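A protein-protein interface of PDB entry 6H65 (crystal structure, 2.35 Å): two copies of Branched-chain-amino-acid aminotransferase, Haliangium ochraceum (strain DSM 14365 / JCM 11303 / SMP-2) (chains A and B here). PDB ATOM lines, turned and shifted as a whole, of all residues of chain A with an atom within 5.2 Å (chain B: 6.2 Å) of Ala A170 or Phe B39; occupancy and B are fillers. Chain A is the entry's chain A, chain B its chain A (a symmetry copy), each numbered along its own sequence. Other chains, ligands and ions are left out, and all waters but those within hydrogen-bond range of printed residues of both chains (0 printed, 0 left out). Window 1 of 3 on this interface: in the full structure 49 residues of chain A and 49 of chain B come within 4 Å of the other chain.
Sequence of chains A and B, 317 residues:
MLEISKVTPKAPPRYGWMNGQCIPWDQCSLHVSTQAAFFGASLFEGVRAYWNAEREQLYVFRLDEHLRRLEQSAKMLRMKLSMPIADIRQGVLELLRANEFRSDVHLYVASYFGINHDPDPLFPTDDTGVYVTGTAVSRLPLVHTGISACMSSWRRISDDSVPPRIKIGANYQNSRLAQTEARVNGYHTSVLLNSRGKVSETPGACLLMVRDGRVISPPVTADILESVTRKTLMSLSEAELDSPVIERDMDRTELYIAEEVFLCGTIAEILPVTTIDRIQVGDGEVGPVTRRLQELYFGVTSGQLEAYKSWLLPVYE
NH1 of Arg A176 is in hydrogen-bond range of OE1 of Gln B35 (3.2 Å).
The side-chain amide oxygen (OD1) of Asn B116 sits at hydrogen-bond distance from the side-chain amide nitrogen (NE2) of Gln B35, 2.9 Å away. O of Gln B35 is in hydrogen-bond range of N of Ala B41 (3.4 Å). O of Gly B40 lies within hydrogen-bond range of N of Ala B170, 3.0 Å away. The backbone NH (N) of Gly B169 lies close to the backbone carbonyl oxygen (O) of Gly B40, 3.5 Å away. The backbone carbonyl oxygen of Ser B42 is in hydrogen-bond range of the backbone NH of Gly B169, at 2.9 Å. The backbone carbonyl oxygen (O) of Gly A40 lies within hydrogen-bond range of the backbone NH (N) of Ala A170 (3.0 Å).
Among the printed residues, merely in contact across the chains: Phe A39 with Gly B40, Phe A39 with Gly B169, Phe A39 with Ala B170, Phe A39 with Tyr B172, Gly A40 with Phe B38, Gly A40 with Phe B39, Gly A40 with Gly B40, Ile A168 with Gln B173, Gly A169 with Phe B38, Gly A169 with Phe B39, Ala A170 with Phe B39, Ala A170 with Ala B170, Tyr A172 with Phe B39, Tyr A172 with Leu B122, Arg A176 with Phe B39, Arg A176 with Pro B121 and Arg A176 with Leu B122.
Of the printed residues of chain B, Ala A170 touches Phe B39 and Ala B170. Phe B39 touches just these residues of chain A: Gly A40 (3.7 Å), Gly A169 (3.7 Å), Ala A170 (3.8 Å), Tyr A172 (3.5 Å) and Arg A176 (3.96 Å). Of the printed residues of chain A, Gln B173 touches Ile A168. Of the printed residues of chain A, Leu B122 touches Tyr A172 and Arg A176. Of the printed residues of chain A, Phe B38 touches Gly A40 and Gly A169. Printed residues of chain A within 4 Å of Gly B169: Phe A39. The nearest printed residue of chain B that does not touch Gly A169 is Gly B40 (5.3 Å).
Hydrophobic or aromatic side chains of chain A that line the printed part of chain B: Phe A39, Ile A168, Ala A170 and Tyr A172. Of the 17 printed residues of chain B, 10 touch a printed residue of chain A. Hydrophobic or aromatic side chains of chain B within 4 Å of the printed part of chain A: Phe B39, Leu B122, Ala B170 and Tyr B172. Among the printed residues, 18 pairs touch across the chains. Among the printed residues, no Asp or Glu carboxylate lies within 4 Å of a Lys or Arg side-chain nitrogen of the other chain.
Phe A39 touches Gly B40, and with the chains exchanged Gly A40 touches Phe B39. Phe A39 touches Ala B170, and with the chains exchanged Ala A170 touches Phe B39. Phe A39 touches Tyr B172, and with the chains exchanged Tyr A172 touches Phe B39. Gly A40 touches its own counterpart, Gly B40. Positions printed for both chains: 39, 40, 41, 169, 170, 171, 172 and 173. Of the 18 pairs that touch across the chains among the printed residues, 10 have their exchanged pair printed and touching as well.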
ATOM      1  N   PHE A  39      -2.423  -9.277 -15.949  1.00  0.00           N
ATOM      2  CA  PHE A  39      -2.682  -8.762 -14.611  1.00  0.00           C
ATOM      3  C   PHE A  39      -3.271  -7.356 -14.655  1.00  0.00           C
ATOM      4  O   PHE A  39      -3.668  -6.827 -13.632  1.00  0.00           O
ATOM      5  CB  PHE A  39      -1.401  -8.674 -13.787  1.00  0.00           C
ATOM      6  CG  PHE A  39      -0.782 -10.016 -13.466  1.00  0.00           C
ATOM      7  CD1 PHE A  39      -1.444 -10.919 -12.648  1.00  0.00           C
ATOM      8  CD2 PHE A  39       0.479 -10.360 -13.949  1.00  0.00           C
ATOM      9  CE1 PHE A  39      -0.838 -12.120 -12.312  1.00  0.00           C
ATOM     10  CE2 PHE A  39       1.072 -11.571 -13.634  1.00  0.00           C
ATOM     11  CZ  PHE A  39       0.414 -12.437 -12.799  1.00  0.00           C
ATOM     12  N   GLY A  40      -3.311  -6.739 -15.831  1.00  0.00           N
ATOM     13  CA  GLY A  40      -3.557  -5.310 -15.892  1.00  0.00           C
ATOM     14  C   GLY A  40      -2.407  -4.493 -15.277  1.00  0.00           C
ATOM     15  O   GLY A  40      -2.663  -3.467 -14.655  1.00  0.00           O
ATOM     16  N   ALA A  41      -1.173  -4.985 -15.401  1.00  0.00           N
ATOM     17  CA  ALA A  41      -0.017  -4.334 -14.812  1.00  0.00           C
ATOM     18  C   ALA A  41       0.510  -3.272 -15.780  1.00  0.00           C
ATOM     19  O   ALA A  41       1.561  -3.417 -16.376  1.00  0.00           O
ATOM     20  CB  ALA A  41       1.039  -5.376 -14.463  1.00  0.00           C
ATOM     21  N   ILE A 168      -3.086   2.234 -11.694  1.00  0.00           N
ATOM     22  CA  ILE A 168      -2.672   1.055 -12.442  1.00  0.00           C
ATOM     23  C   ILE A 168      -3.920   0.274 -12.873  1.00  0.00           C
ATOM     24  O   ILE A 168      -4.889   0.205 -12.131  1.00  0.00           O
ATOM     25  CB  ILE A 168      -1.722   0.193 -11.587  1.00  0.00           C
ATOM     26  CG1 ILE A 168      -1.053  -0.890 -12.419  1.00  0.00           C
ATOM     27  CG2 ILE A 168      -2.352  -0.384 -10.327  1.00  0.00           C
ATOM     28  CD1 ILE A 168      -0.061  -1.706 -11.653  1.00  0.00           C
ATOM     29  N   GLY A 169      -3.916  -0.260 -14.097  1.00  0.00           N
ATOM     30  CA  GLY A 169      -5.023  -1.018 -14.639  1.00  0.00           C
ATOM     31  C   GLY A 169      -5.704  -1.882 -13.580  1.00  0.00           C
ATOM     32  O   GLY A 169      -6.910  -1.780 -13.369  1.00  0.00           O
ATOM     33  N   ALA A 170      -4.888  -2.686 -12.871  1.00  0.00           N
ATOM     34  CA  ALA A 170      -5.357  -3.691 -11.940  1.00  0.00           C
ATOM     35  C   ALA A 170      -6.228  -3.088 -10.833  1.00  0.00           C
ATOM     36  O   ALA A 170      -7.188  -3.727 -10.385  1.00  0.00           O
ATOM     37  CB  ALA A 170      -4.203  -4.496 -11.443  1.00  0.00           C
ATOM     38  N   ASN A 171      -6.002  -1.828 -10.477  1.00  0.00           N
ATOM     39  CA  ASN A 171      -6.655  -1.256  -9.303  1.00  0.00           C
ATOM     40  C   ASN A 171      -8.089  -0.828  -9.592  1.00  0.00           C
ATOM     41  O   ASN A 171      -8.713  -0.218  -8.739  1.00  0.00           O
ATOM     42  CB  ASN A 171      -5.898  -0.035  -8.749  1.00  0.00           C
ATOM     43  CG  ASN A 171      -5.234  -0.196  -7.390  1.00  0.00           C
ATOM     44  OD1 ASN A 171      -5.896  -0.623  -6.423  1.00  0.00           O
ATOM     45  ND2 ASN A 171      -3.990   0.275  -7.269  1.00  0.00           N
ATOM     46  N   TYR A 172      -8.594  -1.114 -10.783  1.00  0.00           N
ATOM     47  CA  TYR A 172      -9.917  -0.643 -11.123  1.00  0.00           C
ATOM     48  C   TYR A 172     -11.012  -1.663 -10.830  1.00  0.00           C
ATOM     49  O   TYR A 172     -12.181  -1.373 -11.017  1.00  0.00           O
ATOM     50  CB  TYR A 172      -9.917  -0.191 -12.571  1.00  0.00           C
ATOM     51  CG  TYR A 172      -9.399   1.217 -12.666  1.00  0.00           C
ATOM     52  CD1 TYR A 172      -8.037   1.489 -12.734  1.00  0.00           C
ATOM     53  CD2 TYR A 172     -10.292   2.282 -12.614  1.00  0.00           C
ATOM     54  CE1 TYR A 172      -7.589   2.804 -12.760  1.00  0.00           C
ATOM     55  CE2 TYR A 172      -9.860   3.597 -12.689  1.00  0.00           C
ATOM     56  CZ  TYR A 172      -8.504   3.855 -12.759  1.00  0.00           C
ATOM     57  OH  TYR A 172      -8.111   5.159 -12.847  1.00  0.00           O
ATOM     58  N   GLN A 173     -10.648  -2.845 -10.364  1.00  0.00           N
ATOM     59  CA  GLN A 173     -11.677  -3.796 -10.033  1.00  0.00           C
ATOM     60  C   GLN A 173     -12.648  -3.209  -8.990  1.00  0.00           C
ATOM     61  O   GLN A 173     -13.858  -3.262  -9.128  1.00  0.00           O
ATOM     62  CB  GLN A 173     -11.006  -5.143  -9.774  1.00  0.00           C
ATOM     63  CG  GLN A 173     -12.000  -6.261  -9.499  1.00  0.00           C
ATOM     64  CD  GLN A 173     -12.783  -6.697 -10.709  1.00  0.00           C
ATOM     65  OE1 GLN A 173     -12.683  -6.109 -11.790  1.00  0.00           O
ATOM     66  NE2 GLN A 173     -13.566  -7.749 -10.502  1.00  0.00           N
ATOM     67  N   ARG A 176     -14.880  -0.914 -10.832  1.00  0.00           N
ATOM     68  CA  ARG A 176     -15.787  -1.589 -11.741  1.00  0.00           C
ATOM     69  C   ARG A 176     -16.979  -2.158 -10.973  1.00  0.00           C
ATOM     70  O   ARG A 176     -18.135  -2.093 -11.433  1.00  0.00           O
ATOM     71  CB  ARG A 176     -15.060  -2.616 -12.601  1.00  0.00           C
ATOM     72  CG  ARG A 176     -14.103  -1.999 -13.622  1.00  0.00           C
ATOM     73  CD  ARG A 176     -13.080  -2.824 -14.392  1.00  0.00           C
ATOM     74  NE  ARG A 176     -13.654  -4.017 -15.008  1.00  0.00           N
ATOM     75  CZ  ARG A 176     -14.542  -4.078 -15.986  1.00  0.00           C
ATOM     76  NH1 ARG A 176     -14.830  -2.990 -16.692  1.00  0.00           N
ATOM     77  NH2 ARG A 176     -15.157  -5.230 -16.210  1.00  0.00           N
ATOM     78  N   THR B  34      -8.822  -3.446 -24.975  1.00  0.00           N
ATOM     79  CA  THR B  34      -9.779  -4.380 -24.410  1.00  0.00           C
ATOM     80  C   THR B  34      -9.765  -4.281 -22.887  1.00  0.00           C
ATOM     81  O   THR B  34      -8.731  -3.938 -22.303  1.00  0.00           O
ATOM     82  CB  THR B  34      -9.508  -5.846 -24.783  1.00  0.00           C
ATOM     83  OG1 THR B  34      -8.293  -6.270 -24.180  1.00  0.00           O
ATOM     84  CG2 THR B  34      -9.568  -6.116 -26.275  1.00  0.00           C
ATOM     85  N   GLN B  35     -10.891  -4.630 -22.241  1.00  0.00           N
ATOM     86  CA  GLN B  35     -10.927  -4.549 -20.805  1.00  0.00           C
ATOM     87  C   GLN B  35      -9.915  -5.546 -20.248  1.00  0.00           C
ATOM     88  O   GLN B  35      -9.303  -5.327 -19.193  1.00  0.00           O
ATOM     89  CB  GLN B  35     -12.328  -4.744 -20.247  1.00  0.00           C
ATOM     90  CG  GLN B  35     -13.326  -3.702 -20.711  1.00  0.00           C
ATOM     91  CD  GLN B  35     -14.701  -3.805 -20.083  1.00  0.00           C
ATOM     92  OE1 GLN B  35     -15.025  -4.713 -19.360  1.00  0.00           O
ATOM     93  NE2 GLN B  35     -15.560  -2.863 -20.385  1.00  0.00           N
ATOM     94  N   ALA B  36      -9.714  -6.648 -20.982  1.00  0.00           N
ATOM     95  CA  ALA B  36      -8.812  -7.673 -20.484  1.00  0.00           C
ATOM     96  C   ALA B  36      -7.392  -7.114 -20.394  1.00  0.00           C
ATOM     97  O   ALA B  36      -6.787  -7.140 -19.327  1.00  0.00           O
ATOM     98  CB  ALA B  36      -8.898  -8.902 -21.353  1.00  0.00           C
ATOM     99  N   ALA B  37      -6.888  -6.582 -21.510  1.00  0.00           N
ATOM    100  CA  ALA B  37      -5.537  -6.034 -21.588  1.00  0.00           C
ATOM    101  C   ALA B  37      -5.349  -4.885 -20.599  1.00  0.00           C
ATOM    102  O   ALA B  37      -4.357  -4.825 -19.898  1.00  0.00           O
ATOM    103  CB  ALA B  37      -5.230  -5.590 -23.005  1.00  0.00           C
ATOM    104  N   PHE B  38      -6.328  -3.985 -20.523  1.00  0.00           N
ATOM    105  CA  PHE B  38      -6.152  -2.719 -19.828  1.00  0.00           C
ATOM    106  C   PHE B  38      -6.325  -2.897 -18.318  1.00  0.00           C
ATOM    107  O   PHE B  38      -5.501  -2.407 -17.536  1.00  0.00           O
ATOM    108  CB  PHE B  38      -7.093  -1.687 -20.432  1.00  0.00           C
ATOM    109  CG  PHE B  38      -6.876  -0.308 -19.903  1.00  0.00           C
ATOM    110  CD1 PHE B  38      -5.908   0.512 -20.464  1.00  0.00           C
ATOM    111  CD2 PHE B  38      -7.587   0.147 -18.804  1.00  0.00           C
ATOM    112  CE1 PHE B  38      -5.683   1.790 -19.959  1.00  0.00           C
ATOM    113  CE2 PHE B  38      -7.374   1.427 -18.305  1.00  0.00           C
ATOM    114  CZ  PHE B  38      -6.418   2.246 -18.881  1.00  0.00           C
ATOM    115  N   PHE B  39      -7.387  -3.613 -17.903  1.00  0.00           N
ATOM    116  CA  PHE B  39      -7.745  -3.721 -16.495  1.00  0.00           C
ATOM    117  C   PHE B  39      -7.280  -5.045 -15.897  1.00  0.00           C
ATOM    118  O   PHE B  39      -7.382  -5.245 -14.700  1.00  0.00           O
ATOM    119  CB  PHE B  39      -9.256  -3.657 -16.294  1.00  0.00           C
ATOM    120  CG  PHE B  39      -9.868  -2.319 -16.646  1.00  0.00           C
ATOM    121  CD1 PHE B  39      -9.554  -1.187 -15.911  1.00  0.00           C
ATOM    122  CD2 PHE B  39     -10.787  -2.201 -17.687  1.00  0.00           C
ATOM    123  CE1 PHE B  39     -10.169   0.020 -16.206  1.00  0.00           C
ATOM    124  CE2 PHE B  39     -11.381  -0.990 -17.998  1.00  0.00           C
ATOM    125  CZ  PHE B  39     -11.081   0.112 -17.239  1.00  0.00           C
ATOM    126  N   GLY B  40      -6.790  -5.960 -16.727  1.00  0.00           N
ATOM    127  CA  GLY B  40      -6.630  -7.331 -16.282  1.00  0.00           C
ATOM    128  C   GLY B  40      -7.980  -8.016 -16.005  1.00  0.00           C
ATOM    129  O   GLY B  40      -8.072  -8.813 -15.076  1.00  0.00           O
ATOM    130  N   ALA B  41      -9.016  -7.655 -16.766  1.00  0.00           N
ATOM    131  CA  ALA B  41     -10.350  -8.189 -16.560  1.00  0.00           C
ATOM    132  C   ALA B  41     -10.488  -9.507 -17.325  1.00  0.00           C
ATOM    133  O   ALA B  41     -11.181  -9.598 -18.320  1.00  0.00           O
ATOM    134  CB  ALA B  41     -11.388  -7.158 -16.989  1.00  0.00           C
ATOM    135  N   SER B  42      -9.716 -10.503 -16.896  1.00  0.00           N
ATOM    136  CA  SER B  42      -9.784 -11.877 -17.322  1.00  0.00           C
ATOM    137  C   SER B  42     -10.037 -12.696 -16.079  1.00  0.00           C
ATOM    138  O   SER B  42      -9.243 -12.681 -15.132  1.00  0.00           O
ATOM    139  CB  SER B  42      -8.504 -12.353 -17.914  1.00  0.00           C
ATOM    140  OG  SER B  42      -8.132 -11.564 -19.002  1.00  0.00           O
ATOM    141  N   ASN B 116     -15.082  -2.413 -25.440  1.00  0.00           N
ATOM    142  CA  ASN B 116     -16.177  -1.777 -24.748  1.00  0.00           C
ATOM    143  C   ASN B 116     -17.351  -1.491 -25.673  1.00  0.00           C
ATOM    144  O   ASN B 116     -17.185  -1.002 -26.783  1.00  0.00           O
ATOM    145  CB  ASN B 116     -15.747  -0.385 -24.334  1.00  0.00           C
ATOM    146  CG  ASN B 116     -15.430  -0.355 -22.874  1.00  0.00           C
ATOM    147  OD1 ASN B 116     -16.337  -0.576 -22.071  1.00  0.00           O
ATOM    148  ND2 ASN B 116     -14.187  -0.015 -22.560  1.00  0.00           N
ATOM    149  N   PRO B 121     -16.355   3.418 -19.222  1.00  0.00           N
ATOM    150  CA  PRO B 121     -15.294   2.407 -19.344  1.00  0.00           C
ATOM    151  C   PRO B 121     -15.202   1.449 -18.156  1.00  0.00           C
ATOM    152  O   PRO B 121     -14.503   0.427 -18.194  1.00  0.00           O
ATOM    153  CB  PRO B 121     -14.022   3.224 -19.461  1.00  0.00           C
ATOM    154  CG  PRO B 121     -14.358   4.523 -18.738  1.00  0.00           C
ATOM    155  CD  PRO B 121     -15.848   4.760 -18.907  1.00  0.00           C
ATOM    156  N   LEU B 122     -15.958   1.774 -17.096  1.00  0.00           N
ATOM    157  CA  LEU B 122     -15.912   0.950 -15.903  1.00  0.00           C
ATOM    158  C   LEU B 122     -17.080  -0.044 -15.853  1.00  0.00           C
ATOM    159  O   LEU B 122     -17.196  -0.761 -14.870  1.00  0.00           O
ATOM    160  CB  LEU B 122     -15.968   1.888 -14.707  1.00  0.00           C
ATOM    161  CG  LEU B 122     -14.721   2.731 -14.546  1.00  0.00           C
ATOM    162  CD1 LEU B 122     -14.974   4.019 -13.784  1.00  0.00           C
ATOM    163  CD2 LEU B 122     -13.582   1.869 -14.046  1.00  0.00           C
ATOM    164  N   GLY B 169      -7.370 -11.657 -13.183  1.00  0.00           N
ATOM    165  CA  GLY B 169      -6.093 -11.011 -13.398  1.00  0.00           C
ATOM    166  C   GLY B 169      -5.866  -9.846 -12.436  1.00  0.00           C
ATOM    167  O   GLY B 169      -4.867  -9.812 -11.721  1.00  0.00           O
ATOM    168  N   ALA B 170      -6.852  -8.931 -12.387  1.00  0.00           N
ATOM    169  CA  ALA B 170      -6.754  -7.680 -11.663  1.00  0.00           C
ATOM    170  C   ALA B 170      -6.466  -7.898 -10.174  1.00  0.00           C
ATOM    171  O   ALA B 170      -5.744  -7.102  -9.560  1.00  0.00           O
ATOM    172  CB  ALA B 170      -7.957  -6.843 -11.938  1.00  0.00           C
ATOM    173  N   ASN B 171      -6.898  -9.023  -9.612  1.00  0.00           N
ATOM    174  CA  ASN B 171      -6.833  -9.206  -8.164  1.00  0.00           C
ATOM    175  C   ASN B 171      -5.439  -9.607  -7.696  1.00  0.00           C
ATOM    176  O   ASN B 171      -5.269  -9.917  -6.528  1.00  0.00           O
ATOM    177  CB  ASN B 171      -7.827 -10.270  -7.665  1.00  0.00           C
ATOM    178  CG  ASN B 171      -8.988  -9.781  -6.812  1.00  0.00           C
ATOM    179  OD1 ASN B 171      -8.766  -9.064  -5.816  1.00  0.00           O
ATOM    180  ND2 ASN B 171     -10.194 -10.277  -7.098  1.00  0.00           N
ATOM    181  N   TYR B 172      -4.466  -9.631  -8.594  1.00  0.00           N
ATOM    182  CA  TYR B 172      -3.154 -10.094  -8.204  1.00  0.00           C
ATOM    183  C   TYR B 172      -2.221  -8.967  -7.774  1.00  0.00           C
ATOM    184  O   TYR B 172      -1.102  -9.224  -7.367  1.00  0.00           O
ATOM    185  CB  TYR B 172      -2.576 -10.928  -9.332  1.00  0.00           C
ATOM    186  CG  TYR B 172      -3.093 -12.336  -9.241  1.00  0.00           C
ATOM    187  CD1 TYR B 172      -4.315 -12.701  -9.795  1.00  0.00           C
ATOM    188  CD2 TYR B 172      -2.372 -13.289  -8.528  1.00  0.00           C
ATOM    189  CE1 TYR B 172      -4.792 -13.997  -9.642  1.00  0.00           C
ATOM    190  CE2 TYR B 172      -2.813 -14.597  -8.411  1.00  0.00           C
ATOM    191  CZ  TYR B 172      -4.028 -14.948  -8.967  1.00  0.00           C
ATOM    192  OH  TYR B 172      -4.428 -16.247  -8.848  1.00  0.00           O
ATOM    193  N   GLN B 173      -2.673  -7.727  -7.850  1.00  0.00           N
ATOM    194  CA  GLN B 173      -1.820  -6.660  -7.396  1.00  0.00           C
ATOM    195  C   GLN B 173      -1.413  -6.875  -5.925  1.00  0.00           C
ATOM    196  O   GLN B 173      -0.255  -6.787  -5.552  1.00  0.00           O
ATOM    197  CB  GLN B 173      -2.453  -5.338  -7.826  1.00  0.00           C
ATOM    198  CG  GLN B 173      -1.598  -4.128  -7.480  1.00  0.00           C
ATOM    199  CD  GLN B 173      -0.355  -3.996  -8.319  1.00  0.00           C
ATOM    200  OE1 GLN B 173      -0.030  -4.865  -9.134  1.00  0.00           O
ATOM    201  NE2 GLN B 173       0.333  -2.881  -8.104  1.00  0.00           N
